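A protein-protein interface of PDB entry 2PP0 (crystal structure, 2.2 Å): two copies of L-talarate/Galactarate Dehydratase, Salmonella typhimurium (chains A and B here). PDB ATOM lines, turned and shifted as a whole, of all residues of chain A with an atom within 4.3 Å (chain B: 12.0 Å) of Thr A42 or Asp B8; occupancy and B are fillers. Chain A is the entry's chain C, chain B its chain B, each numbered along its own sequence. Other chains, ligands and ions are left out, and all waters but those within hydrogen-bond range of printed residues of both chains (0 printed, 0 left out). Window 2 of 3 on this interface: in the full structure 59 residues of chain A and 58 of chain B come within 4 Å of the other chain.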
ATOM      1  N   LEU A  40       5.738  -4.755   0.136  1.00  0.00           N
ATOM      2  CA  LEU A  40       4.537  -4.267  -0.537  1.00  0.00           C
ATOM      3  C   LEU A  40       4.940  -3.007  -1.304  1.00  0.00           C
ATOM      4  O   LEU A  40       5.142  -1.947  -0.706  1.00  0.00           O
ATOM      5  CB  LEU A  40       3.445  -3.928   0.484  1.00  0.00           C
ATOM      6  CG  LEU A  40       2.908  -5.066   1.360  1.00  0.00           C
ATOM      7  CD1 LEU A  40       1.967  -4.492   2.420  1.00  0.00           C
ATOM      8  CD2 LEU A  40       2.187  -6.087   0.497  1.00  0.00           C
ATOM      9  N   ALA A  41       5.064  -3.133  -2.622  1.00  0.00           N
ATOM     10  CA  ALA A  41       5.464  -2.014  -3.478  1.00  0.00           C
ATOM     11  C   ALA A  41       4.557  -0.806  -3.323  1.00  0.00           C
ATOM     12  O   ALA A  41       5.012   0.337  -3.388  1.00  0.00           O
ATOM     13  CB  ALA A  41       5.485  -2.454  -4.939  1.00  0.00           C
ATOM     14  N   THR A  42       3.267  -1.057  -3.138  1.00  0.00           N
ATOM     15  CA  THR A  42       2.319   0.029  -2.963  1.00  0.00           C
ATOM     16  C   THR A  42       1.937   0.126  -1.494  1.00  0.00           C
ATOM     17  O   THR A  42       1.192  -0.711  -0.991  1.00  0.00           O
ATOM     18  CB  THR A  42       1.044  -0.201  -3.801  1.00  0.00           C
ATOM     19  OG1 THR A  42       1.382  -0.184  -5.195  1.00  0.00           O
ATOM     20  CG2 THR A  42       0.009   0.881  -3.515  1.00  0.00           C
ATOM     21  N   PRO A  43       2.459   1.141  -0.782  1.00  0.00           N
ATOM     22  CA  PRO A  43       2.135   1.306   0.640  1.00  0.00           C
ATOM     23  C   PRO A  43       0.627   1.172   0.822  1.00  0.00           C
ATOM     24  O   PRO A  43      -0.149   1.707   0.027  1.00  0.00           O
ATOM     25  CB  PRO A  43       2.648   2.708   0.944  1.00  0.00           C
ATOM     26  CG  PRO A  43       3.869   2.795   0.063  1.00  0.00           C
ATOM     27  CD  PRO A  43       3.365   2.210  -1.244  1.00  0.00           C
ATOM     28  N   VAL A  44       0.219   0.456   1.865  1.00  0.00           N
ATOM     29  CA  VAL A  44      -1.197   0.206   2.128  1.00  0.00           C
ATOM     30  C   VAL A  44      -1.762   1.007   3.298  1.00  0.00           C
ATOM     31  O   VAL A  44      -1.172   1.052   4.378  1.00  0.00           O
ATOM     32  CB  VAL A  44      -1.419  -1.305   2.390  1.00  0.00           C
ATOM     33  CG1 VAL A  44      -2.887  -1.587   2.705  1.00  0.00           C
ATOM     34  CG2 VAL A  44      -0.963  -2.103   1.179  1.00  0.00           C
ATOM     35  N   HIS A 173      -6.125   4.059   0.457  1.00  0.00           N
ATOM     36  CA  HIS A 173      -5.068   4.767  -0.261  1.00  0.00           C
ATOM     37  C   HIS A 173      -5.357   4.676  -1.764  1.00  0.00           C
ATOM     38  O   HIS A 173      -4.647   5.262  -2.582  1.00  0.00           O
ATOM     39  CB  HIS A 173      -3.704   4.134   0.042  1.00  0.00           C
ATOM     40  CG  HIS A 173      -3.588   2.708  -0.401  1.00  0.00           C
ATOM     41  ND1 HIS A 173      -3.281   2.351  -1.697  1.00  0.00           N
ATOM     42  CD2 HIS A 173      -3.778   1.547   0.271  1.00  0.00           C
ATOM     43  CE1 HIS A 173      -3.287   1.033  -1.804  1.00  0.00           C
ATOM     44  NE2 HIS A 173      -3.586   0.522  -0.623  1.00  0.00           N
ATOM     45  N   GLN A 178      -9.963   3.653  -9.239  1.00  0.00           N
ATOM     46  CA  GLN A 178      -9.160   2.435  -9.232  1.00  0.00           C
ATOM     47  C   GLN A 178      -9.876   1.335  -8.450  1.00  0.00           C
ATOM     48  O   GLN A 178      -9.800   0.158  -8.811  1.00  0.00           O
ATOM     49  CB  GLN A 178      -7.782   2.709  -8.624  1.00  0.00           C
ATOM     50  CG  GLN A 178      -6.826   1.518  -8.667  1.00  0.00           C
ATOM     51  CD  GLN A 178      -6.680   0.928 -10.063  1.00  0.00           C
ATOM     52  OE1 GLN A 178      -7.386  -0.015 -10.431  1.00  0.00           O
ATOM     53  NE2 GLN A 178      -5.769   1.489 -10.852  1.00  0.00           N
ATOM     54  N   SER B   4       7.751  -7.544  -5.449  1.00  0.00           N
ATOM     55  CA  SER B   4       6.609  -7.020  -4.638  1.00  0.00           C
ATOM     56  C   SER B   4       5.457  -8.013  -4.529  1.00  0.00           C
ATOM     57  O   SER B   4       5.199  -8.786  -5.454  1.00  0.00           O
ATOM     58  CB  SER B   4       6.080  -5.717  -5.243  1.00  0.00           C
ATOM     59  OG  SER B   4       4.967  -5.237  -4.501  1.00  0.00           O
ATOM     60  N   ALA B   5       4.761  -7.974  -3.395  1.00  0.00           N
ATOM     61  CA  ALA B   5       3.633  -8.863  -3.150  1.00  0.00           C
ATOM     62  C   ALA B   5       2.291  -8.197  -3.450  1.00  0.00           C
ATOM     63  O   ALA B   5       1.243  -8.835  -3.350  1.00  0.00           O
ATOM     64  CB  ALA B   5       3.658  -9.347  -1.706  1.00  0.00           C
ATOM     65  N   ASN B   6       2.320  -6.915  -3.817  1.00  0.00           N
ATOM     66  CA  ASN B   6       1.087  -6.186  -4.126  1.00  0.00           C
ATOM     67  C   ASN B   6       1.313  -5.150  -5.228  1.00  0.00           C
ATOM     68  O   ASN B   6       2.431  -4.990  -5.720  1.00  0.00           O
ATOM     69  CB  ASN B   6       0.554  -5.489  -2.867  1.00  0.00           C
ATOM     70  CG  ASN B   6       1.242  -4.160  -2.588  1.00  0.00           C
ATOM     71  OD1 ASN B   6       2.429  -3.982  -2.883  1.00  0.00           O
ATOM     72  ND2 ASN B   6       0.500  -3.222  -2.001  1.00  0.00           N
ATOM     73  N   SER B   7       0.244  -4.452  -5.607  1.00  0.00           N
ATOM     74  CA  SER B   7       0.307  -3.423  -6.647  1.00  0.00           C
ATOM     75  C   SER B   7      -0.764  -2.362  -6.403  1.00  0.00           C
ATOM     76  O   SER B   7      -1.510  -2.437  -5.423  1.00  0.00           O
ATOM     77  CB  SER B   7       0.088  -4.049  -8.026  1.00  0.00           C
ATOM     78  OG  SER B   7      -1.232  -4.554  -8.155  1.00  0.00           O
ATOM     79  N   ASP B   8      -0.843  -1.378  -7.297  1.00  0.00           N
ATOM     80  CA  ASP B   8      -1.837  -0.315  -7.171  1.00  0.00           C
ATOM     81  C   ASP B   8      -3.247  -0.844  -7.420  1.00  0.00           C
ATOM     82  O   ASP B   8      -4.231  -0.250  -6.976  1.00  0.00           O
ATOM     83  CB  ASP B   8      -1.549   0.825  -8.153  1.00  0.00           C
ATOM     84  CG  ASP B   8      -0.271   1.573  -7.825  1.00  0.00           C
ATOM     85  OD1 ASP B   8       0.088   1.650  -6.630  1.00  0.00           O
ATOM     86  OD2 ASP B   8       0.366   2.102  -8.764  1.00  0.00           O
ATOM     87  N   ALA B   9      -3.344  -1.954  -8.141  1.00  0.00           N
ATOM     88  CA  ALA B   9      -4.643  -2.556  -8.432  1.00  0.00           C
ATOM     89  C   ALA B   9      -4.807  -3.809  -7.574  1.00  0.00           C
ATOM     90  O   ALA B   9      -4.610  -3.775  -6.359  1.00  0.00           O
ATOM     91  CB  ALA B   9      -4.737  -2.908  -9.915  1.00  0.00           C
ATOM     92  N   VAL B  10      -5.171  -4.912  -8.213  1.00  0.00           N
ATOM     93  CA  VAL B  10      -5.343  -6.180  -7.518  1.00  0.00           C
ATOM     94  C   VAL B  10      -4.980  -7.280  -8.509  1.00  0.00           C
ATOM     95  O   VAL B  10      -5.304  -7.182  -9.694  1.00  0.00           O
ATOM     96  CB  VAL B  10      -6.807  -6.365  -7.037  1.00  0.00           C
ATOM     97  CG1 VAL B  10      -7.753  -6.308  -8.223  1.00  0.00           C
ATOM     98  CG2 VAL B  10      -6.952  -7.688  -6.294  1.00  0.00           C
ATOM     99  N   THR B  11      -4.299  -8.318  -8.036  1.00  0.00           N
ATOM    100  CA  THR B  11      -3.905  -9.406  -8.921  1.00  0.00           C
ATOM    101  C   THR B  11      -4.311 -10.770  -8.377  1.00  0.00           C
ATOM    102  O   THR B  11      -4.319 -11.000  -7.165  1.00  0.00           O
ATOM    103  CB  THR B  11      -2.376  -9.413  -9.169  1.00  0.00           C
ATOM    104  OG1 THR B  11      -1.692  -9.747  -7.956  1.00  0.00           O
ATOM    105  CG2 THR B  11      -1.907  -8.047  -9.642  1.00  0.00           C
ATOM    106  N   TYR B  12      -4.644 -11.669  -9.296  1.00  0.00           N
ATOM    107  CA  TYR B  12      -5.057 -13.020  -8.961  1.00  0.00           C
ATOM    108  C   TYR B  12      -4.159 -14.033  -9.658  1.00  0.00           C
ATOM    109  O   TYR B  12      -3.994 -13.998 -10.879  1.00  0.00           O
ATOM    110  CB  TYR B  12      -6.510 -13.236  -9.385  1.00  0.00           C
ATOM    111  CG  TYR B  12      -7.498 -12.470  -8.537  1.00  0.00           C
ATOM    112  CD1 TYR B  12      -7.956 -12.996  -7.328  1.00  0.00           C
ATOM    113  CD2 TYR B  12      -7.944 -11.205  -8.920  1.00  0.00           C
ATOM    114  CE1 TYR B  12      -8.831 -12.286  -6.520  1.00  0.00           C
ATOM    115  CE2 TYR B  12      -8.821 -10.481  -8.115  1.00  0.00           C
ATOM    116  CZ  TYR B  12      -9.260 -11.031  -6.917  1.00  0.00           C
ATOM    117  OH  TYR B  12     -10.127 -10.335  -6.113  1.00  0.00           O
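The side-chain amide nitrogen of Asn B6 is in hydrogen-bond range of the backbone carbonyl oxygen of Thr A42 (2.8 Å).
OG1 of Thr A42 is in hydrogen-bond range of OD1 of Asp B8, 2.7 Å away.
OG of Ser B4 is in hydrogen-bond range of N of Ala A41 (2.8 Å).
OD1 of Asn B6 sits at hydrogen-bond distance from N of Ala A41 (2.8 Å).
The side-chain hydroxyl of Ser B4 lies within hydrogen-bond range of the backbone carbonyl oxygen of Asn B6 (2.8 Å).
The side-chain hydroxyl (OG) of Ser B7 lies close to the backbone NH (N) of Ala B9, 3.3 Å away.
Leu A40 touches Ser B4.
Leu A40 touches Asn B6.
Thr A42 touches Ser B7.
Val A44 touches Asn B6.
Gln A178 touches Asp B8.
Gln A178 touches Ala B9 (OE1 to CB, 3.96 Å).
Thr A42 touches just these residues of chain B: Asn B6 (2.8 Å), Ser B7 (3.3 Å) and Asp B8 (2.7 Å).
Of chain A, only Thr A42 (2.7 Å) and Gln A178 (3.6 Å) come within 4 Å of Asp B8.
Of chain B, only Ser B4 (3.9 Å) and Asn B6 (3.1 Å) come within 4 Å of Leu A40.
Printed residues of chain B within 4 Å of Ala A41: Ser B4 (2.8 Å) and Asn B6 (2.8 Å).
No residue of chain B comes within 4 Å of Pro A43.
Of chain B, only Asn B6 comes within 4 Å of Val A44.
Gln A178 touches just these residues of chain B: Asp B8 and Ala B9.
Of the printed residues of chain A, Ser B7 touches Thr A42 (3.3 Å).
Of the printed residues of chain A, Ala B9 touches Gln A178 (3.96 Å).
His A173 touches none of the printed residues of chain B.
Thr B11 touches none of the printed residues of chain A.
The nearest residue of chain B that does not touch Thr A42 is Ser B4 (4.7 Å).
The nearest printed residue of chain A that does not touch Ser B4 is Thr A42 (4.7 Å).
Of the 9 printed residues of chain B, 5 touch a printed residue of chain A.
Printed residues of chain B that touch a printed residue of chain A: Ser B4, Asn B6, Ser B7, Asp B8 and Ala B9.
Hydrophobic or aromatic side chains of chain B that line the printed part of chain A: Ala B9.
Among the printed residues, no Asp or Glu carboxylate lies within 4 Å of a Lys or Arg side-chain nitrogen of the other chain.
No position is printed for both chains.
Of the 10 pairs that touch across the chains among the printed residues, none has its exchanged pair printed and touching as well.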
